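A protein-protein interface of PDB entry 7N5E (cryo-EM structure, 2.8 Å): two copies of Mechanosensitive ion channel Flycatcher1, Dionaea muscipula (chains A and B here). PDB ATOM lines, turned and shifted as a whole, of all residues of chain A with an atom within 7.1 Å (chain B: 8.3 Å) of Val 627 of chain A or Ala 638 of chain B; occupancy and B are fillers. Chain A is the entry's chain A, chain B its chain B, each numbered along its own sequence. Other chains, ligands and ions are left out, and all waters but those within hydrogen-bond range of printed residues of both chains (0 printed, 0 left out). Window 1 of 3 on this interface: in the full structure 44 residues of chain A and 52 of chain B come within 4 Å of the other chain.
The backbone carbonyl oxygen of Lys 626 of chain A lies within hydrogen-bond range of the backbone NH of Asn 641 of chain B (2.9 Å).
The backbone NH (N) of Lys 626 of chain A lies within hydrogen-bond range of the side-chain hydroxyl (OG) of Ser 645 of chain B (2.9 Å).
The backbone carbonyl oxygen (O) of Ile 639 of chain B is in hydrogen-bond range of the backbone NH (N) of Tyr 628 of chain A, 3.0 Å away.
OH of Tyr 628 of chain A is in hydrogen-bond range of NH1 of Arg 644 of chain B (3.0 Å).
The backbone carbonyl oxygen (O) of Pro 593 of chain B lies within hydrogen-bond range of the guanidinium group (NH1) of Arg 644 of chain B, 3.3 Å away.
OG of Ser 645 of chain B is in hydrogen-bond range of O of Asn 641 of chain B, at 2.7 Å.
The backbone carbonyl oxygen (O) of Thr 617 of chain A is in hydrogen-bond range of the backbone NH (N) of Tyr 629 of chain A (3.0 Å).
N of Val 601 of chain B lies within hydrogen-bond range of O of Gly 640 of chain B (2.8 Å).
NZ of Lys 621 of chain A lies within salt-bridge range of OE2 of Glu 625 of chain A.
The backbone carbonyl oxygen (O) of Phe 619 of chain A lies within hydrogen-bond range of the backbone NH (N) of Val 627 of chain A.
CB of Ser 645 of chain B touches O of Lys 624 of chain A, at 3.7 Å.
Pro 646 of chain B touches Lys 624 of chain A (CD to O, 3.5 Å).
Val 601 of chain B touches Glu 625 of chain A (CG2 to OE1, 3.6 Å).
CA of Gly 640 of chain B touches OE2 of Glu 625 of chain A, 3.7 Å away.
Phe 642 of chain B touches Glu 625 of chain A (CE2 to OE1, 3.2 Å).
Gly 640 of chain B touches Lys 626 of chain A.
Lys 626 of chain A touches Arg 644 of chain B.
CA of Ala 638 of chain B touches O of Tyr 628 of chain A (3.3 Å).
Ala 638 of chain B touches Tyr 629 of chain A (CB to CD1, 3.6 Å).
Lys 637 of chain B touches Pro 630 of chain A (O to CD, 3.6 Å).
Printed residues of chain B within 4 Å of Lys 624 of chain A: Ser 645 and Pro 646.
Of the printed residues of chain B, Val 627 of chain A touches Ala 638 (3.98 Å) and Ile 639 (3.6 Å).
Of the printed residues of chain B, Tyr 629 of chain A touches Ala 638.
Of the printed residues of chain A, Cys 635 of chain B touches Pro 630.
Printed residues of chain A within 4 Å of Ala 638 of chain B: Val 627 (3.98 Å), Tyr 628 (3.3 Å) and Tyr 629 (3.6 Å).
The nearest printed residue of chain B that does not touch Tyr 629 of chain A is Ile 639 of chain B (5.2 Å).
Printed residues of chain B that touch a printed residue of chain A: Pro 593, Val 601, Cys 635, Thr 636, Lys 637, Ala 638, Ile 639, Gly 640, Asn 641, Phe 642, Arg 644, Ser 645 and Pro 646.
Along chain B the printed residues that touch a printed residue of chain A span positions 593 to 646.
Printed residues of chain A that touch a printed residue of chain B: Lys 624, Glu 625, Lys 626, Val 627, Tyr 628, Tyr 629, Pro 630 and Ile 633.
Hydrophobic or aromatic side chains of chain A within 4 Å of the printed part of chain B: Val 627, Tyr 628, Tyr 629, Pro 630 and Ile 633.
Along chain A the printed residues that touch a printed residue of chain B span positions 624 to 633.
Among the printed residues, no Asp or Glu carboxylate lies within 4 Å of a Lys or Arg side-chain nitrogen of the other chain.
Position printed for both chains: 633.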
ATOM      1  N   MET A 607      19.335 -35.948  12.331  1.00  0.00           N
ATOM      2  CA  MET A 607      20.744 -35.632  12.382  1.00  0.00           C
ATOM      3  C   MET A 607      21.511 -36.481  13.366  1.00  0.00           C
ATOM      4  O   MET A 607      21.005 -36.858  14.413  1.00  0.00           O
ATOM      5  CB  MET A 607      20.935 -34.189  12.752  1.00  0.00           C
ATOM      6  CG  MET A 607      20.266 -33.213  11.837  1.00  0.00           C
ATOM      7  SD  MET A 607      20.661 -31.523  12.199  1.00  0.00           S
ATOM      8  CE  MET A 607      19.684 -31.239  13.611  1.00  0.00           C
ATOM      9  N   GLU A 610      27.518 -35.407  16.426  1.00  0.00           N
ATOM     10  CA  GLU A 610      28.927 -35.639  16.259  1.00  0.00           C
ATOM     11  C   GLU A 610      29.697 -35.282  17.497  1.00  0.00           C
ATOM     12  O   GLU A 610      30.539 -36.042  17.946  1.00  0.00           O
ATOM     13  CB  GLU A 610      29.476 -34.834  15.106  1.00  0.00           C
ATOM     14  CG  GLU A 610      30.907 -35.125  14.834  1.00  0.00           C
ATOM     15  CD  GLU A 610      31.464 -34.364  13.701  1.00  0.00           C
ATOM     16  OE1 GLU A 610      30.736 -33.689  13.029  1.00  0.00           O
ATOM     17  OE2 GLU A 610      32.662 -34.408  13.512  1.00  0.00           O
ATOM     18  N   THR A 616      27.834 -25.266  22.177  1.00  0.00           N
ATOM     19  CA  THR A 616      27.256 -25.801  20.950  1.00  0.00           C
ATOM     20  C   THR A 616      27.191 -27.306  20.920  1.00  0.00           C
ATOM     21  O   THR A 616      27.967 -27.989  21.592  1.00  0.00           O
ATOM     22  CB  THR A 616      28.065 -25.398  19.707  1.00  0.00           C
ATOM     23  OG1 THR A 616      29.372 -25.965  19.787  1.00  0.00           O
ATOM     24  CG2 THR A 616      28.179 -23.942  19.596  1.00  0.00           C
ATOM     25  N   THR A 617      26.341 -27.804  20.045  1.00  0.00           N
ATOM     26  CA  THR A 617      26.293 -29.205  19.697  1.00  0.00           C
ATOM     27  C   THR A 617      26.536 -29.281  18.207  1.00  0.00           C
ATOM     28  O   THR A 617      26.042 -28.445  17.448  1.00  0.00           O
ATOM     29  CB  THR A 617      24.963 -29.869  20.066  1.00  0.00           C
ATOM     30  OG1 THR A 617      24.759 -29.782  21.482  1.00  0.00           O
ATOM     31  CG2 THR A 617      24.996 -31.347  19.662  1.00  0.00           C
ATOM     32  N   VAL A 618      27.355 -30.217  17.778  1.00  0.00           N
ATOM     33  CA  VAL A 618      27.630 -30.345  16.364  1.00  0.00           C
ATOM     34  C   VAL A 618      26.946 -31.567  15.822  1.00  0.00           C
ATOM     35  O   VAL A 618      27.132 -32.664  16.345  1.00  0.00           O
ATOM     36  CB  VAL A 618      29.121 -30.412  16.105  1.00  0.00           C
ATOM     37  CG1 VAL A 618      29.389 -30.556  14.641  1.00  0.00           C
ATOM     38  CG2 VAL A 618      29.751 -29.188  16.632  1.00  0.00           C
ATOM     39  N   PHE A 619      26.155 -31.368  14.784  1.00  0.00           N
ATOM     40  CA  PHE A 619      25.370 -32.419  14.162  1.00  0.00           C
ATOM     41  C   PHE A 619      25.685 -32.667  12.699  1.00  0.00           C
ATOM     42  O   PHE A 619      26.079 -31.762  11.978  1.00  0.00           O
ATOM     43  CB  PHE A 619      23.901 -32.057  14.183  1.00  0.00           C
ATOM     44  CG  PHE A 619      23.240 -31.956  15.463  1.00  0.00           C
ATOM     45  CD1 PHE A 619      23.168 -30.768  16.113  1.00  0.00           C
ATOM     46  CD2 PHE A 619      22.644 -33.037  16.010  1.00  0.00           C
ATOM     47  CE1 PHE A 619      22.521 -30.670  17.293  1.00  0.00           C
ATOM     48  CE2 PHE A 619      21.995 -32.936  17.192  1.00  0.00           C
ATOM     49  CZ  PHE A 619      21.940 -31.754  17.831  1.00  0.00           C
ATOM     50  N   LEU A 620      25.454 -33.877  12.226  1.00  0.00           N
ATOM     51  CA  LEU A 620      25.560 -34.164  10.800  1.00  0.00           C
ATOM     52  C   LEU A 620      24.210 -34.460  10.203  1.00  0.00           C
ATOM     53  O   LEU A 620      23.467 -35.319  10.673  1.00  0.00           O
ATOM     54  CB  LEU A 620      26.463 -35.365  10.510  1.00  0.00           C
ATOM     55  CG  LEU A 620      27.946 -35.271  10.831  1.00  0.00           C
ATOM     56  CD1 LEU A 620      28.561 -36.617  10.641  1.00  0.00           C
ATOM     57  CD2 LEU A 620      28.625 -34.300   9.893  1.00  0.00           C
ATOM     58  N   LYS A 621      23.901 -33.790   9.124  1.00  0.00           N
ATOM     59  CA  LYS A 621      22.622 -33.985   8.460  1.00  0.00           C
ATOM     60  C   LYS A 621      22.658 -35.238   7.622  1.00  0.00           C
ATOM     61  O   LYS A 621      23.695 -35.882   7.510  1.00  0.00           O
ATOM     62  CB  LYS A 621      22.269 -32.782   7.622  1.00  0.00           C
ATOM     63  CG  LYS A 621      22.036 -31.538   8.429  1.00  0.00           C
ATOM     64  CD  LYS A 621      21.778 -30.329   7.548  1.00  0.00           C
ATOM     65  CE  LYS A 621      20.379 -30.276   6.992  1.00  0.00           C
ATOM     66  NZ  LYS A 621      20.212 -29.090   6.104  1.00  0.00           N
ATOM     67  N   LYS A 624      25.419 -35.371   5.320  1.00  0.00           N
ATOM     68  CA  LYS A 624      26.627 -35.166   6.075  1.00  0.00           C
ATOM     69  C   LYS A 624      27.112 -33.736   6.127  1.00  0.00           C
ATOM     70  O   LYS A 624      28.276 -33.491   6.426  1.00  0.00           O
ATOM     71  CB  LYS A 624      27.749 -36.019   5.525  1.00  0.00           C
ATOM     72  CG  LYS A 624      27.410 -37.458   5.245  1.00  0.00           C
ATOM     73  CD  LYS A 624      27.124 -38.249   6.487  1.00  0.00           C
ATOM     74  CE  LYS A 624      26.679 -39.653   6.129  1.00  0.00           C
ATOM     75  NZ  LYS A 624      27.695 -40.394   5.326  1.00  0.00           N
ATOM     76  N   GLU A 625      26.223 -32.779   5.941  1.00  0.00           N
ATOM     77  CA  GLU A 625      26.608 -31.405   6.180  1.00  0.00           C
ATOM     78  C   GLU A 625      26.839 -31.247   7.667  1.00  0.00           C
ATOM     79  O   GLU A 625      26.029 -31.707   8.475  1.00  0.00           O
ATOM     80  CB  GLU A 625      25.506 -30.451   5.761  1.00  0.00           C
ATOM     81  CG  GLU A 625      25.799 -28.962   5.936  1.00  0.00           C
ATOM     82  CD  GLU A 625      24.617 -28.138   5.526  1.00  0.00           C
ATOM     83  OE1 GLU A 625      24.400 -27.984   4.359  1.00  0.00           O
ATOM     84  OE2 GLU A 625      23.911 -27.676   6.393  1.00  0.00           O
ATOM     85  N   LYS A 626      27.919 -30.588   8.047  1.00  0.00           N
ATOM     86  CA  LYS A 626      28.199 -30.336   9.451  1.00  0.00           C
ATOM     87  C   LYS A 626      27.499 -29.088   9.918  1.00  0.00           C
ATOM     88  O   LYS A 626      27.663 -28.022   9.337  1.00  0.00           O
ATOM     89  CB  LYS A 626      29.691 -30.193   9.676  1.00  0.00           C
ATOM     90  CG  LYS A 626      30.088 -30.114  11.123  1.00  0.00           C
ATOM     91  CD  LYS A 626      31.537 -29.768  11.287  1.00  0.00           C
ATOM     92  CE  LYS A 626      32.492 -30.879  10.950  1.00  0.00           C
ATOM     93  NZ  LYS A 626      32.576 -31.875  11.985  1.00  0.00           N
ATOM     94  N   VAL A 627      26.735 -29.208  10.991  1.00  0.00           N
ATOM     95  CA  VAL A 627      25.956 -28.111  11.533  1.00  0.00           C
ATOM     96  C   VAL A 627      26.281 -27.733  12.955  1.00  0.00           C
ATOM     97  O   VAL A 627      26.221 -28.558  13.861  1.00  0.00           O
ATOM     98  CB  VAL A 627      24.474 -28.487  11.488  1.00  0.00           C
ATOM     99  CG1 VAL A 627      23.614 -27.387  12.081  1.00  0.00           C
ATOM    100  CG2 VAL A 627      24.088 -28.761  10.094  1.00  0.00           C
ATOM    101  N   TYR A 628      26.562 -26.466  13.156  1.00  0.00           N
ATOM    102  CA  TYR A 628      26.832 -25.941  14.476  1.00  0.00           C
ATOM    103  C   TYR A 628      25.546 -25.392  15.014  1.00  0.00           C
ATOM    104  O   TYR A 628      24.985 -24.441  14.473  1.00  0.00           O
ATOM    105  CB  TYR A 628      27.900 -24.886  14.393  1.00  0.00           C
ATOM    106  CG  TYR A 628      29.175 -25.469  14.048  1.00  0.00           C
ATOM    107  CD1 TYR A 628      29.504 -25.708  12.743  1.00  0.00           C
ATOM    108  CD2 TYR A 628      30.028 -25.777  15.026  1.00  0.00           C
ATOM    109  CE1 TYR A 628      30.691 -26.267  12.452  1.00  0.00           C
ATOM    110  CE2 TYR A 628      31.213 -26.329  14.732  1.00  0.00           C
ATOM    111  CZ  TYR A 628      31.542 -26.575  13.462  1.00  0.00           C
ATOM    112  OH  TYR A 628      32.748 -27.128  13.187  1.00  0.00           O
ATOM    113  N   TYR A 629      25.058 -25.991  16.081  1.00  0.00           N
ATOM    114  CA  TYR A 629      23.754 -25.659  16.599  1.00  0.00           C
ATOM    115  C   TYR A 629      23.855 -25.203  18.062  1.00  0.00           C
ATOM    116  O   TYR A 629      24.157 -26.030  18.922  1.00  0.00           O
ATOM    117  CB  TYR A 629      22.929 -26.911  16.505  1.00  0.00           C
ATOM    118  CG  TYR A 629      21.537 -26.715  16.475  1.00  0.00           C
ATOM    119  CD1 TYR A 629      20.913 -27.096  15.344  1.00  0.00           C
ATOM    120  CD2 TYR A 629      20.855 -26.151  17.477  1.00  0.00           C
ATOM    121  CE1 TYR A 629      19.616 -26.930  15.210  1.00  0.00           C
ATOM    122  CE2 TYR A 629      19.536 -25.976  17.339  1.00  0.00           C
ATOM    123  CZ  TYR A 629      18.925 -26.369  16.204  1.00  0.00           C
ATOM    124  OH  TYR A 629      17.606 -26.197  16.061  1.00  0.00           O
ATOM    125  N   PRO A 630      23.685 -23.917  18.393  1.00  0.00           N
ATOM    126  CA  PRO A 630      23.845 -23.367  19.719  1.00  0.00           C
ATOM    127  C   PRO A 630      22.981 -24.049  20.743  1.00  0.00           C
ATOM    128  O   PRO A 630      21.793 -24.286  20.506  1.00  0.00           O
ATOM    129  CB  PRO A 630      23.379 -21.938  19.525  1.00  0.00           C
ATOM    130  CG  PRO A 630      23.625 -21.662  18.095  1.00  0.00           C
ATOM    131  CD  PRO A 630      23.325 -22.936  17.395  1.00  0.00           C
ATOM    132  N   ILE A 633      19.586 -22.480  21.999  1.00  0.00           N
ATOM    133  CA  ILE A 633      18.416 -22.667  21.179  1.00  0.00           C
ATOM    134  C   ILE A 633      17.918 -24.063  21.337  1.00  0.00           C
ATOM    135  O   ILE A 633      16.727 -24.325  21.410  1.00  0.00           O
ATOM    136  CB  ILE A 633      18.723 -22.419  19.736  1.00  0.00           C
ATOM    137  CG1 ILE A 633      19.076 -21.024  19.619  1.00  0.00           C
ATOM    138  CG2 ILE A 633      17.548 -22.821  18.861  1.00  0.00           C
ATOM    139  CD1 ILE A 633      19.638 -20.674  18.373  1.00  0.00           C
ATOM    140  N   PHE B 587      30.935 -15.516  20.075  1.00  0.00           N
ATOM    141  CA  PHE B 587      30.633 -16.213  18.841  1.00  0.00           C
ATOM    142  C   PHE B 587      31.847 -16.324  17.936  1.00  0.00           C
ATOM    143  O   PHE B 587      32.179 -17.400  17.432  1.00  0.00           O
ATOM    144  CB  PHE B 587      29.523 -15.489  18.140  1.00  0.00           C
ATOM    145  CG  PHE B 587      29.134 -15.988  16.839  1.00  0.00           C
ATOM    146  CD1 PHE B 587      28.347 -17.061  16.729  1.00  0.00           C
ATOM    147  CD2 PHE B 587      29.532 -15.351  15.714  1.00  0.00           C
ATOM    148  CE1 PHE B 587      27.960 -17.502  15.522  1.00  0.00           C
ATOM    149  CE2 PHE B 587      29.155 -15.790  14.502  1.00  0.00           C
ATOM    150  CZ  PHE B 587      28.369 -16.867  14.407  1.00  0.00           C
ATOM    151  N   PRO B 593      32.127 -21.100  14.397  1.00  0.00           N
ATOM    152  CA  PRO B 593      31.487 -21.967  13.418  1.00  0.00           C
ATOM    153  C   PRO B 593      32.077 -21.933  12.013  1.00  0.00           C
ATOM    154  O   PRO B 593      31.786 -22.815  11.209  1.00  0.00           O
ATOM    155  CB  PRO B 593      30.063 -21.448  13.412  1.00  0.00           C
ATOM    156  CG  PRO B 593      30.171 -20.037  13.870  1.00  0.00           C
ATOM    157  CD  PRO B 593      31.271 -20.016  14.858  1.00  0.00           C
ATOM    158  N   CYS B 600      29.330 -21.720   3.821  1.00  0.00           N
ATOM    159  CA  CYS B 600      28.424 -21.994   4.920  1.00  0.00           C
ATOM    160  C   CYS B 600      26.978 -21.944   4.518  1.00  0.00           C
ATOM    161  O   CYS B 600      26.635 -21.337   3.513  1.00  0.00           O
ATOM    162  CB  CYS B 600      28.659 -20.980   6.011  1.00  0.00           C
ATOM    163  SG  CYS B 600      30.297 -21.034   6.622  1.00  0.00           S
ATOM    164  N   VAL B 601      26.112 -22.593   5.272  1.00  0.00           N
ATOM    165  CA  VAL B 601      24.710 -22.519   4.923  1.00  0.00           C
ATOM    166  C   VAL B 601      23.907 -21.901   6.053  1.00  0.00           C
ATOM    167  O   VAL B 601      23.853 -22.435   7.162  1.00  0.00           O
ATOM    168  CB  VAL B 601      24.172 -23.906   4.621  1.00  0.00           C
ATOM    169  CG1 VAL B 601      22.732 -23.797   4.188  1.00  0.00           C
ATOM    170  CG2 VAL B 601      25.045 -24.559   3.618  1.00  0.00           C
ATOM    171  N   ILE B 602      23.293 -20.761   5.783  1.00  0.00           N
ATOM    172  CA  ILE B 602      22.523 -20.064   6.802  1.00  0.00           C
ATOM    173  C   ILE B 602      21.104 -19.861   6.324  1.00  0.00           C
ATOM    174  O   ILE B 602      20.874 -19.207   5.320  1.00  0.00           O
ATOM    175  CB  ILE B 602      23.205 -18.738   7.139  1.00  0.00           C
ATOM    176  CG1 ILE B 602      24.626 -19.048   7.640  1.00  0.00           C
ATOM    177  CG2 ILE B 602      22.404 -17.957   8.161  1.00  0.00           C
ATOM    178  CD1 ILE B 602      25.505 -17.893   7.826  1.00  0.00           C
ATOM    179  N   ASP B 603      20.136 -20.424   7.024  1.00  0.00           N
ATOM    180  CA  ASP B 603      18.731 -20.336   6.634  1.00  0.00           C
ATOM    181  C   ASP B 603      18.500 -20.777   5.193  1.00  0.00           C
ATOM    182  O   ASP B 603      17.707 -20.190   4.462  1.00  0.00           O
ATOM    183  CB  ASP B 603      18.196 -18.925   6.836  1.00  0.00           C
ATOM    184  CG  ASP B 603      18.179 -18.502   8.302  1.00  0.00           C
ATOM    185  OD1 ASP B 603      17.990 -19.341   9.158  1.00  0.00           O
ATOM    186  OD2 ASP B 603      18.356 -17.326   8.565  1.00  0.00           O
ATOM    187  N   GLY B 604      19.213 -21.808   4.783  1.00  0.00           N
ATOM    188  CA  GLY B 604      19.097 -22.370   3.446  1.00  0.00           C
ATOM    189  C   GLY B 604      19.940 -21.662   2.381  1.00  0.00           C
ATOM    190  O   GLY B 604      19.996 -22.124   1.240  1.00  0.00           O
ATOM    191  N   ILE B 633      22.777 -11.752  15.232  1.00  0.00           N
ATOM    192  CA  ILE B 633      21.713 -12.607  14.750  1.00  0.00           C
ATOM    193  C   ILE B 633      22.326 -13.958  14.386  1.00  0.00           C
ATOM    194  O   ILE B 633      21.708 -14.993  14.576  1.00  0.00           O
ATOM    195  CB  ILE B 633      20.864 -11.982  13.624  1.00  0.00           C
ATOM    196  CG1 ILE B 633      21.653 -11.758  12.314  1.00  0.00           C
ATOM    197  CG2 ILE B 633      20.324 -10.655  14.162  1.00  0.00           C
ATOM    198  CD1 ILE B 633      20.779 -11.370  11.102  1.00  0.00           C
ATOM    199  N   LEU B 634      23.578 -13.983  13.909  1.00  0.00           N
ATOM    200  CA  LEU B 634      24.195 -15.273  13.584  1.00  0.00           C
ATOM    201  C   LEU B 634      24.368 -16.124  14.826  1.00  0.00           C
ATOM    202  O   LEU B 634      24.284 -17.350  14.765  1.00  0.00           O
ATOM    203  CB  LEU B 634      25.558 -15.121  12.939  1.00  0.00           C
ATOM    204  CG  LEU B 634      25.614 -14.555  11.577  1.00  0.00           C
ATOM    205  CD1 LEU B 634      27.028 -14.349  11.218  1.00  0.00           C
ATOM    206  CD2 LEU B 634      25.005 -15.483  10.599  1.00  0.00           C
ATOM    207  N   CYS B 635      24.523 -15.477  15.968  1.00  0.00           N
ATOM    208  CA  CYS B 635      24.679 -16.143  17.246  1.00  0.00           C
ATOM    209  C   CYS B 635      23.485 -16.994  17.613  1.00  0.00           C
ATOM    210  O   CYS B 635      23.569 -17.784  18.548  1.00  0.00           O
ATOM    211  CB  CYS B 635      24.806 -15.138  18.381  1.00  0.00           C
ATOM    212  SG  CYS B 635      26.254 -14.158  18.379  1.00  0.00           S
ATOM    213  N   THR B 636      22.355 -16.811  16.944  1.00  0.00           N
ATOM    214  CA  THR B 636      21.178 -17.571  17.252  1.00  0.00           C
ATOM    215  C   THR B 636      20.757 -18.468  16.102  1.00  0.00           C
ATOM    216  O   THR B 636      19.590 -18.850  16.010  1.00  0.00           O
ATOM    217  CB  THR B 636      19.991 -16.684  17.617  1.00  0.00           C
ATOM    218  OG1 THR B 636      19.658 -15.846  16.532  1.00  0.00           O
ATOM    219  CG2 THR B 636      20.381 -15.824  18.775  1.00  0.00           C
ATOM    220  N   LYS B 637      21.651 -18.737  15.166  1.00  0.00           N
ATOM    221  CA  LYS B 637      21.302 -19.583  14.042  1.00  0.00           C
ATOM    222  C   LYS B 637      22.091 -20.862  13.990  1.00  0.00           C
ATOM    223  O   LYS B 637      23.221 -20.929  14.463  1.00  0.00           O
ATOM    224  CB  LYS B 637      21.510 -18.823  12.752  1.00  0.00           C
ATOM    225  CG  LYS B 637      20.603 -17.674  12.626  1.00  0.00           C
ATOM    226  CD  LYS B 637      20.796 -16.945  11.342  1.00  0.00           C
ATOM    227  CE  LYS B 637      19.928 -15.723  11.285  1.00  0.00           C
ATOM    228  NZ  LYS B 637      18.498 -16.084  11.139  1.00  0.00           N
ATOM    229  N   ALA B 638      21.504 -21.884  13.387  1.00  0.00           N
ATOM    230  CA  ALA B 638      22.236 -23.111  13.143  1.00  0.00           C
ATOM    231  C   ALA B 638      22.994 -22.910  11.851  1.00  0.00           C
ATOM    232  O   ALA B 638      22.402 -22.560  10.832  1.00  0.00           O
ATOM    233  CB  ALA B 638      21.312 -24.296  13.077  1.00  0.00           C
ATOM    234  N   ILE B 639      24.298 -23.071  11.891  1.00  0.00           N
ATOM    235  CA  ILE B 639      25.109 -22.776  10.726  1.00  0.00           C
ATOM    236  C   ILE B 639      25.772 -23.990  10.118  1.00  0.00           C
ATOM    237  O   ILE B 639      26.544 -24.683  10.780  1.00  0.00           O
ATOM    238  CB  ILE B 639      26.170 -21.723  11.119  1.00  0.00           C
ATOM    239  CG1 ILE B 639      25.429 -20.449  11.608  1.00  0.00           C
ATOM    240  CG2 ILE B 639      27.120 -21.431   9.968  1.00  0.00           C
ATOM    241  CD1 ILE B 639      26.275 -19.383  12.208  1.00  0.00           C
ATOM    242  N   GLY B 640      25.491 -24.250   8.845  1.00  0.00           N
ATOM    243  CA  GLY B 640      26.122 -25.373   8.177  1.00  0.00           C
ATOM    244  C   GLY B 640      27.492 -24.926   7.727  1.00  0.00           C
ATOM    245  O   GLY B 640      27.644 -23.790   7.303  1.00  0.00           O
ATOM    246  N   ASN B 641      28.447 -25.824   7.668  1.00  0.00           N
ATOM    247  CA  ASN B 641      29.772 -25.494   7.170  1.00  0.00           C
ATOM    248  C   ASN B 641      30.264 -26.601   6.259  1.00  0.00           C
ATOM    249  O   ASN B 641      30.610 -27.682   6.725  1.00  0.00           O
ATOM    250  CB  ASN B 641      30.725 -25.227   8.315  1.00  0.00           C
ATOM    251  CG  ASN B 641      32.042 -24.767   7.854  1.00  0.00           C
ATOM    252  OD1 ASN B 641      32.596 -25.316   6.893  1.00  0.00           O
ATOM    253  ND2 ASN B 641      32.591 -23.773   8.505  1.00  0.00           N
ATOM    254  N   PHE B 642      30.277 -26.345   4.954  1.00  0.00           N
ATOM    255  CA  PHE B 642      30.666 -27.356   3.986  1.00  0.00           C
ATOM    256  C   PHE B 642      32.146 -27.613   4.033  1.00  0.00           C
ATOM    257  O   PHE B 642      32.586 -28.744   3.955  1.00  0.00           O
ATOM    258  CB  PHE B 642      30.343 -26.926   2.578  1.00  0.00           C
ATOM    259  CG  PHE B 642      28.925 -26.896   2.178  1.00  0.00           C
ATOM    260  CD1 PHE B 642      28.560 -25.999   1.266  1.00  0.00           C
ATOM    261  CD2 PHE B 642      27.980 -27.743   2.653  1.00  0.00           C
ATOM    262  CE1 PHE B 642      27.298 -25.915   0.812  1.00  0.00           C
ATOM    263  CE2 PHE B 642      26.715 -27.668   2.201  1.00  0.00           C
ATOM    264  CZ  PHE B 642      26.376 -26.755   1.281  1.00  0.00           C
ATOM    265  N   ARG B 644      34.210 -27.760   6.397  1.00  0.00           N
ATOM    266  CA  ARG B 644      34.555 -28.666   7.473  1.00  0.00           C
ATOM    267  C   ARG B 644      33.853 -30.023   7.410  1.00  0.00           C
ATOM    268  O   ARG B 644      34.104 -30.881   8.258  1.00  0.00           O
ATOM    269  CB  ARG B 644      34.216 -28.019   8.799  1.00  0.00           C
ATOM    270  CG  ARG B 644      35.014 -26.790   9.143  1.00  0.00           C
ATOM    271  CD  ARG B 644      34.603 -26.226  10.441  1.00  0.00           C
ATOM    272  NE  ARG B 644      35.313 -24.998  10.752  1.00  0.00           N
ATOM    273  CZ  ARG B 644      35.076 -24.218  11.821  1.00  0.00           C
ATOM    274  NH1 ARG B 644      34.180 -24.523  12.694  1.00  0.00           N
ATOM    275  NH2 ARG B 644      35.735 -23.104  12.018  1.00  0.00           N
ATOM    276  N   SER B 645      32.967 -30.215   6.451  1.00  0.00           N
ATOM    277  CA  SER B 645      32.193 -31.434   6.317  1.00  0.00           C
ATOM    278  C   SER B 645      32.985 -32.582   5.688  1.00  0.00           C
ATOM    279  O   SER B 645      33.916 -32.362   4.912  1.00  0.00           O
ATOM    280  CB  SER B 645      30.953 -31.152   5.490  1.00  0.00           C
ATOM    281  OG  SER B 645      30.082 -30.290   6.169  1.00  0.00           O
ATOM    282  N   PRO B 646      32.634 -33.836   5.987  1.00  0.00           N
ATOM    283  CA  PRO B 646      33.145 -35.038   5.394  1.00  0.00           C
ATOM    284  C   PRO B 646      32.513 -35.150   4.035  1.00  0.00           C
ATOM    285  O   PRO B 646      31.631 -34.362   3.722  1.00  0.00           O
ATOM    286  CB  PRO B 646      32.666 -36.112   6.341  1.00  0.00           C
ATOM    287  CG  PRO B 646      31.417 -35.574   6.858  1.00  0.00           C
ATOM    288  CD  PRO B 646      31.654 -34.110   7.029  1.00  0.00           C
